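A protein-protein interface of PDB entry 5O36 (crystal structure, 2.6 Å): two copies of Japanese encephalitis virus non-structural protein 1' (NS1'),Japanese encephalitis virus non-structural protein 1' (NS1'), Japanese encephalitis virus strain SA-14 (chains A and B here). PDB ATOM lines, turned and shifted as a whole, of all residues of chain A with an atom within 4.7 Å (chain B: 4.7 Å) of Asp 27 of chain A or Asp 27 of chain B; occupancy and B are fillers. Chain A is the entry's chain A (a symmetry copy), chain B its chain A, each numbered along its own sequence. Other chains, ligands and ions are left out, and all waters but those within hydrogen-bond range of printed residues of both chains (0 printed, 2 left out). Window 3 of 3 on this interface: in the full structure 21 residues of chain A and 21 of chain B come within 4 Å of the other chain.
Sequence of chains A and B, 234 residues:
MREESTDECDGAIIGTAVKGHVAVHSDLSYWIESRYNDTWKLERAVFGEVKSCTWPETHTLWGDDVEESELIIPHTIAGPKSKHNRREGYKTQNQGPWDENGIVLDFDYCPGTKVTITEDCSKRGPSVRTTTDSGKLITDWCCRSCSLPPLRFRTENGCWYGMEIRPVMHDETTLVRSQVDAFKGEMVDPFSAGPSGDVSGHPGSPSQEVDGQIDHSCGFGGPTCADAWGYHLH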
ATOM      1  N   ILE A  13       9.662 -13.922   2.998  1.00  0.00           N
ATOM      2  CA  ILE A  13       8.771 -12.775   3.320  1.00  0.00           C
ATOM      3  C   ILE A  13       8.616 -11.655   2.243  1.00  0.00           C
ATOM      4  O   ILE A  13       8.346 -10.487   2.552  1.00  0.00           O
ATOM      5  CB  ILE A  13       9.189 -12.201   4.698  1.00  0.00           C
ATOM      6  CG1 ILE A  13      10.715 -11.832   4.763  1.00  0.00           C
ATOM      7  CG2 ILE A  13       8.744 -13.182   5.799  1.00  0.00           C
ATOM      8  CD1 ILE A  13      10.973 -10.346   5.032  1.00  0.00           C
ATOM      9  N   ILE A  14       8.764 -12.041   0.972  1.00  0.00           N
ATOM     10  CA  ILE A  14       8.692 -11.123  -0.144  1.00  0.00           C
ATOM     11  C   ILE A  14       7.555 -11.459  -1.105  1.00  0.00           C
ATOM     12  O   ILE A  14       7.411 -12.600  -1.546  1.00  0.00           O
ATOM     13  CB  ILE A  14      10.000 -11.109  -0.931  1.00  0.00           C
ATOM     14  CG1 ILE A  14      11.157 -10.733  -0.011  1.00  0.00           C
ATOM     15  CG2 ILE A  14       9.919 -10.127  -2.087  1.00  0.00           C
ATOM     16  CD1 ILE A  14      12.488 -10.556  -0.739  1.00  0.00           C
ATOM     17  N   HIS A  25       6.837  -4.424  -5.899  1.00  0.00           N
ATOM     18  CA  HIS A  25       7.854  -5.174  -5.163  1.00  0.00           C
ATOM     19  C   HIS A  25       7.651  -4.870  -3.703  1.00  0.00           C
ATOM     20  O   HIS A  25       7.704  -3.725  -3.308  1.00  0.00           O
ATOM     21  CB  HIS A  25       9.251  -4.739  -5.563  1.00  0.00           C
ATOM     22  CG  HIS A  25       9.664  -5.203  -6.920  1.00  0.00           C
ATOM     23  ND1 HIS A  25       9.302  -4.536  -8.069  1.00  0.00           N
ATOM     24  CD2 HIS A  25      10.397  -6.267  -7.316  1.00  0.00           C
ATOM     25  CE1 HIS A  25       9.827  -5.139  -9.117  1.00  0.00           C
ATOM     26  NE2 HIS A  25      10.488  -6.195  -8.691  1.00  0.00           N
ATOM     27  N   SER A  26       7.396  -5.893  -2.908  1.00  0.00           N
ATOM     28  CA  SER A  26       7.082  -5.690  -1.507  1.00  0.00           C
ATOM     29  C   SER A  26       7.689  -6.751  -0.574  1.00  0.00           C
ATOM     30  O   SER A  26       7.948  -7.896  -0.986  1.00  0.00           O
ATOM     31  CB  SER A  26       5.560  -5.604  -1.300  1.00  0.00           C
ATOM     32  OG  SER A  26       4.946  -6.846  -1.508  1.00  0.00           O
ATOM     33  N   ASP A  27       7.986  -6.323   0.653  1.00  0.00           N
ATOM     34  CA  ASP A  27       8.367  -7.226   1.715  1.00  0.00           C
ATOM     35  C   ASP A  27       7.775  -6.688   2.996  1.00  0.00           C
ATOM     36  O   ASP A  27       6.844  -5.903   2.923  1.00  0.00           O
ATOM     37  CB  ASP A  27       9.873  -7.405   1.778  1.00  0.00           C
ATOM     38  CG  ASP A  27      10.615  -6.157   2.251  1.00  0.00           C
ATOM     39  OD1 ASP A  27      10.050  -5.168   2.767  1.00  0.00           O
ATOM     40  OD2 ASP A  27      11.830  -6.182   2.090  1.00  0.00           O
ATOM     41  N   LEU A  28       8.252  -7.121   4.160  1.00  0.00           N
ATOM     42  CA  LEU A  28       7.656  -6.646   5.405  1.00  0.00           C
ATOM     43  C   LEU A  28       7.875  -5.166   5.710  1.00  0.00           C
ATOM     44  O   LEU A  28       7.029  -4.607   6.373  1.00  0.00           O
ATOM     45  CB  LEU A  28       8.053  -7.475   6.588  1.00  0.00           C
ATOM     46  CG  LEU A  28       7.480  -8.869   6.599  1.00  0.00           C
ATOM     47  CD1 LEU A  28       8.099  -9.591   7.772  1.00  0.00           C
ATOM     48  CD2 LEU A  28       5.963  -8.885   6.711  1.00  0.00           C
ATOM     49  N   SER A  29       8.926  -4.514   5.226  1.00  0.00           N
ATOM     50  CA  SER A  29       9.027  -3.048   5.414  1.00  0.00           C
ATOM     51  C   SER A  29       8.821  -2.190   4.182  1.00  0.00           C
ATOM     52  O   SER A  29       8.394  -1.048   4.339  1.00  0.00           O
ATOM     53  CB  SER A  29      10.326  -2.621   6.108  1.00  0.00           C
ATOM     54  OG  SER A  29      11.427  -3.321   5.598  1.00  0.00           O
ATOM     55  N   TYR A  30       9.098  -2.704   2.977  1.00  0.00           N
ATOM     56  CA  TYR A  30       9.065  -1.887   1.750  1.00  0.00           C
ATOM     57  C   TYR A  30       7.818  -2.174   0.929  1.00  0.00           C
ATOM     58  O   TYR A  30       7.322  -3.302   0.927  1.00  0.00           O
ATOM     59  CB  TYR A  30      10.263  -2.226   0.906  1.00  0.00           C
ATOM     60  CG  TYR A  30      11.593  -1.740   1.389  1.00  0.00           C
ATOM     61  CD1 TYR A  30      11.797  -1.245   2.700  1.00  0.00           C
ATOM     62  CD2 TYR A  30      12.685  -1.783   0.527  1.00  0.00           C
ATOM     63  CE1 TYR A  30      13.052  -0.794   3.112  1.00  0.00           C
ATOM     64  CE2 TYR A  30      13.943  -1.344   0.925  1.00  0.00           C
ATOM     65  CZ  TYR A  30      14.109  -0.838   2.217  1.00  0.00           C
ATOM     66  OH  TYR A  30      15.314  -0.422   2.613  1.00  0.00           O
ATOM     67  N   LYS A  51      16.618  -0.811   5.512  1.00  0.00           N
ATOM     68  CA  LYS A  51      17.480  -1.945   5.912  1.00  0.00           C
ATOM     69  C   LYS A  51      18.581  -2.158   4.897  1.00  0.00           C
ATOM     70  O   LYS A  51      18.451  -1.753   3.789  1.00  0.00           O
ATOM     71  CB  LYS A  51      16.653  -3.230   6.078  1.00  0.00           C
ATOM     72  CG  LYS A  51      15.599  -3.448   5.009  1.00  0.00           C
ATOM     73  CD  LYS A  51      15.028  -4.859   5.066  1.00  0.00           C
ATOM     74  CE  LYS A  51      14.444  -5.271   3.722  1.00  0.00           C
ATOM     75  NZ  LYS A  51      13.304  -4.380   3.352  1.00  0.00           N
ATOM     76  N   TRP A  55      18.162  -7.282  -2.449  1.00  0.00           N
ATOM     77  CA  TRP A  55      16.841  -7.815  -2.742  1.00  0.00           C
ATOM     78  C   TRP A  55      17.104  -8.954  -3.667  1.00  0.00           C
ATOM     79  O   TRP A  55      17.750  -8.737  -4.683  1.00  0.00           O
ATOM     80  CB  TRP A  55      15.964  -6.780  -3.437  1.00  0.00           C
ATOM     81  CG  TRP A  55      14.502  -7.148  -3.608  1.00  0.00           C
ATOM     82  CD1 TRP A  55      13.968  -8.004  -4.523  1.00  0.00           C
ATOM     83  CD2 TRP A  55      13.405  -6.651  -2.852  1.00  0.00           C
ATOM     84  NE1 TRP A  55      12.595  -8.104  -4.368  1.00  0.00           N
ATOM     85  CE2 TRP A  55      12.217  -7.238  -3.385  1.00  0.00           C
ATOM     86  CE3 TRP A  55      13.295  -5.746  -1.785  1.00  0.00           C
ATOM     87  CZ2 TRP A  55      10.942  -6.970  -2.867  1.00  0.00           C
ATOM     88  CZ3 TRP A  55      12.015  -5.468  -1.278  1.00  0.00           C
ATOM     89  CH2 TRP A  55      10.864  -6.105  -1.808  1.00  0.00           C
ATOM     90  N   ILE B  13       2.135 -14.417   5.119  1.00  0.00           N
ATOM     91  CA  ILE B  13       2.870 -13.162   4.807  1.00  0.00           C
ATOM     92  C   ILE B  13       2.881 -12.040   5.894  1.00  0.00           C
ATOM     93  O   ILE B  13       2.999 -10.845   5.595  1.00  0.00           O
ATOM     94  CB  ILE B  13       2.381 -12.635   3.434  1.00  0.00           C
ATOM     95  CG1 ILE B  13       0.821 -12.465   3.372  1.00  0.00           C
ATOM     96  CG2 ILE B  13       2.948 -13.542   2.326  1.00  0.00           C
ATOM     97  CD1 ILE B  13       0.374 -11.022   3.115  1.00  0.00           C
ATOM     98  N   ILE B  14       2.785 -12.452   7.162  1.00  0.00           N
ATOM     99  CA  ILE B  14       2.738 -11.542   8.285  1.00  0.00           C
ATOM    100  C   ILE B  14       3.909 -11.737   9.244  1.00  0.00           C
ATOM    101  O   ILE B  14       4.200 -12.854   9.676  1.00  0.00           O
ATOM    102  CB  ILE B  14       1.440 -11.703   9.072  1.00  0.00           C
ATOM    103  CG1 ILE B  14       0.244 -11.471   8.154  1.00  0.00           C
ATOM    104  CG2 ILE B  14       1.395 -10.729  10.236  1.00  0.00           C
ATOM    105  CD1 ILE B  14      -1.098 -11.472   8.883  1.00  0.00           C
ATOM    106  N   HIS B  25       3.720  -4.709  14.097  1.00  0.00           N
ATOM    107  CA  HIS B  25       2.807  -5.577  13.354  1.00  0.00           C
ATOM    108  C   HIS B  25       2.969  -5.237  11.896  1.00  0.00           C
ATOM    109  O   HIS B  25       2.769  -4.105  11.511  1.00  0.00           O
ATOM    110  CB  HIS B  25       1.366  -5.328  13.757  1.00  0.00           C
ATOM    111  CG  HIS B  25       1.018  -5.852  15.110  1.00  0.00           C
ATOM    112  ND1 HIS B  25       1.291  -5.154  16.265  1.00  0.00           N
ATOM    113  CD2 HIS B  25       0.427  -7.005  15.497  1.00  0.00           C
ATOM    114  CE1 HIS B  25       0.848  -5.828  17.307  1.00  0.00           C
ATOM    115  NE2 HIS B  25       0.328  -6.957  16.872  1.00  0.00           N
ATOM    116  N   SER B  26       3.353  -6.212  11.094  1.00  0.00           N
ATOM    117  CA  SER B  26       3.637  -5.959   9.695  1.00  0.00           C
ATOM    118  C   SER B  26       3.172  -7.082   8.752  1.00  0.00           C
ATOM    119  O   SER B  26       3.062  -8.254   9.154  1.00  0.00           O
ATOM    120  CB  SER B  26       5.135  -5.676   9.489  1.00  0.00           C
ATOM    121  OG  SER B  26       5.904  -6.831   9.687  1.00  0.00           O
ATOM    122  N   ASP B  27       2.822  -6.685   7.529  1.00  0.00           N
ATOM    123  CA  ASP B  27       2.559  -7.621   6.459  1.00  0.00           C
ATOM    124  C   ASP B  27       3.076  -7.000   5.183  1.00  0.00           C
ATOM    125  O   ASP B  27       3.899  -6.102   5.263  1.00  0.00           O
ATOM    126  CB  ASP B  27       1.088  -7.991   6.394  1.00  0.00           C
ATOM    127  CG  ASP B  27       0.192  -6.845   5.931  1.00  0.00           C
ATOM    128  OD1 ASP B  27       0.625  -5.787   5.424  1.00  0.00           O
ATOM    129  OD2 ASP B  27      -1.010  -7.027   6.091  1.00  0.00           O
ATOM    130  N   LEU B  28       2.658  -7.481   4.015  1.00  0.00           N
ATOM    131  CA  LEU B  28       3.188  -6.923   2.774  1.00  0.00           C
ATOM    132  C   LEU B  28       2.780  -5.481   2.482  1.00  0.00           C
ATOM    133  O   LEU B  28       3.547  -4.813   1.823  1.00  0.00           O
ATOM    134  CB  LEU B  28       2.900  -7.787   1.584  1.00  0.00           C
ATOM    135  CG  LEU B  28       3.647  -9.095   1.562  1.00  0.00           C
ATOM    136  CD1 LEU B  28       3.125  -9.881   0.382  1.00  0.00           C
ATOM    137  CD2 LEU B  28       5.154  -8.916   1.451  1.00  0.00           C
ATOM    138  N   SER B  29       1.654  -4.974   2.970  1.00  0.00           N
ATOM    139  CA  SER B  29       1.366  -3.532   2.795  1.00  0.00           C
ATOM    140  C   SER B  29       1.460  -2.664   4.034  1.00  0.00           C
ATOM    141  O   SER B  29       1.737  -1.476   3.886  1.00  0.00           O
ATOM    142  CB  SER B  29       0.022  -3.269   2.104  1.00  0.00           C
ATOM    143  OG  SER B  29      -0.980  -4.109   2.607  1.00  0.00           O
ATOM    144  N   TYR B  30       1.252  -3.220   5.234  1.00  0.00           N
ATOM    145  CA  TYR B  30       1.180  -2.416   6.467  1.00  0.00           C
ATOM    146  C   TYR B  30       2.455  -2.546   7.287  1.00  0.00           C
ATOM    147  O   TYR B  30       3.091  -3.602   7.280  1.00  0.00           O
ATOM    148  CB  TYR B  30       0.037  -2.913   7.308  1.00  0.00           C
ATOM    149  CG  TYR B  30      -1.346  -2.597   6.829  1.00  0.00           C
ATOM    150  CD1 TYR B  30      -1.612  -2.122   5.521  1.00  0.00           C
ATOM    151  CD2 TYR B  30      -2.422  -2.788   7.690  1.00  0.00           C
ATOM    152  CE1 TYR B  30      -2.914  -1.832   5.113  1.00  0.00           C
ATOM    153  CE2 TYR B  30      -3.726  -2.510   7.294  1.00  0.00           C
ATOM    154  CZ  TYR B  30      -3.956  -2.020   6.007  1.00  0.00           C
ATOM    155  OH  TYR B  30      -5.205  -1.759   5.614  1.00  0.00           O
ATOM    156  N   LYS B  51      -6.450  -2.288   2.711  1.00  0.00           N
ATOM    157  CA  LYS B  51      -7.159  -3.520   2.301  1.00  0.00           C
ATOM    158  C   LYS B  51      -8.224  -3.881   3.314  1.00  0.00           C
ATOM    159  O   LYS B  51      -8.146  -3.472   4.425  1.00  0.00           O
ATOM    160  CB  LYS B  51      -6.174  -4.687   2.125  1.00  0.00           C
ATOM    161  CG  LYS B  51      -5.101  -4.776   3.193  1.00  0.00           C
ATOM    162  CD  LYS B  51      -4.353  -6.102   3.125  1.00  0.00           C
ATOM    163  CE  LYS B  51      -3.720  -6.446   4.465  1.00  0.00           C
ATOM    164  NZ  LYS B  51      -2.704  -5.419   4.843  1.00  0.00           N
ATOM    165  N   TRP B  55      -7.146  -8.970  10.617  1.00  0.00           N
ATOM    166  CA  TRP B  55      -5.767  -9.331  10.906  1.00  0.00           C
ATOM    167  C   TRP B  55      -5.880 -10.501  11.821  1.00  0.00           C
ATOM    168  O   TRP B  55      -6.548 -10.377  12.839  1.00  0.00           O
ATOM    169  CB  TRP B  55      -5.030  -8.197  11.611  1.00  0.00           C
ATOM    170  CG  TRP B  55      -3.532  -8.376  11.779  1.00  0.00           C
ATOM    171  CD1 TRP B  55      -2.893  -9.164  12.687  1.00  0.00           C
ATOM    172  CD2 TRP B  55      -2.509  -7.735  11.028  1.00  0.00           C
ATOM    173  NE1 TRP B  55      -1.518  -9.086  12.532  1.00  0.00           N
ATOM    174  CE2 TRP B  55      -1.255  -8.170  11.557  1.00  0.00           C
ATOM    175  CE3 TRP B  55      -2.516  -6.815   9.968  1.00  0.00           C
ATOM    176  CZ2 TRP B  55      -0.025  -7.735  11.041  1.00  0.00           C
ATOM    177  CZ3 TRP B  55      -1.283  -6.371   9.464  1.00  0.00           C
ATOM    178  CH2 TRP B  55      -0.059  -6.859   9.990  1.00  0.00           C
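Ile 13 of chain A touches Leu 28 of chain B, and with the chains exchanged Leu 28 of chain A touches Ile 13 of chain B.
Ser 26 of chain A touches Leu 28 of chain B, and with the chains exchanged Leu 28 of chain A touches Ser 26 of chain B.
Asp 27 of chain B touches its own counterpart, Asp 27 of chain A.
Asp 27 of chain A touches Leu 28 of chain B, and with the chains exchanged Leu 28 of chain A touches Asp 27 of chain B.
Printed residues of chain B within 4 Å of Ile 13 of chain A: Leu 28 (3.7 Å).
Ile 14 of chain A touches none of the printed residues of chain B.
Of the printed residues of chain B, Ser 26 of chain A touches Leu 28.
Asp 27 of chain A touches just these residues of chain B: Asp 27 and Leu 28.
Printed residues of chain A within 4 Å of Ile 13 of chain B: Leu 28.
Of chain A, only Asp 27 (3.8 Å) and Leu 28 (3.6 Å) come within 4 Å of Asp 27 of chain B.
The nearest printed residue of chain A that does not touch Asp 27 of chain B is Ser 29 of chain A (5.3 Å).
The nearest printed residue of chain A that does not touch Ile 13 of chain B is Ile 13 of chain A (6.0 Å).
The side-chain carboxylate (OD1) of Asp 27 of chain A lies within hydrogen-bond range of the backbone NH (N) of Ser 29 of chain A, 2.8 Å away.
The side-chain carboxylate of Asp 27 of chain B lies within salt-bridge range of the side-chain amino group of Lys 51 of chain B (2.6 Å).
The side-chain carboxylate of Asp 27 of chain A lies within hydrogen-bond range of the backbone NH of Tyr 30 of chain A, 2.6 Å away.
OD1 of Asp 27 of chain B is in hydrogen-bond range of N of Tyr 30 of chain B.
N of Ser 29 of chain B is in hydrogen-bond range of OD1 of Asp 27 of chain B, 2.8 Å away.
The side-chain carboxylate of Asp 27 of chain A is in salt-bridge range of the side-chain amino group of Lys 51 of chain A (2.6 Å).
Of the 10 printed residues of chain B, 4 touch a printed residue of chain A.
Of the 10 printed residues of chain A, 4 touch a printed residue of chain B.
Printed residues of chain A that touch a printed residue of chain B: Ile 13, Ser 26, Asp 27 and Leu 28.
Hydrophobic or aromatic side chains of chain A within 4 Å of the printed part of chain B: Leu 28.
Along chain A the printed residues that touch a printed residue of chain B span positions 13 to 28.
Among the printed residues, 7 pairs touch across the chains.
Among the printed residues, no Asp or Glu carboxylate lies within 4 Å of a Lys or Arg side-chain nitrogen of the other chain.
Among the printed residues, merely in contact across the chains: Leu 28 of chain A with Ser 26 of chain B, Ser 26 of chain A with Leu 28 of chain B, Leu 28 of chain A with Asp 27 of chain B, Asp 27 of chain A with Leu 28 of chain B, Ile 13 of chain A with Leu 28 of chain B, Leu 28 of chain A with Ile 13 of chain B and Asp 27 of chain A with Asp 27 of chain B.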
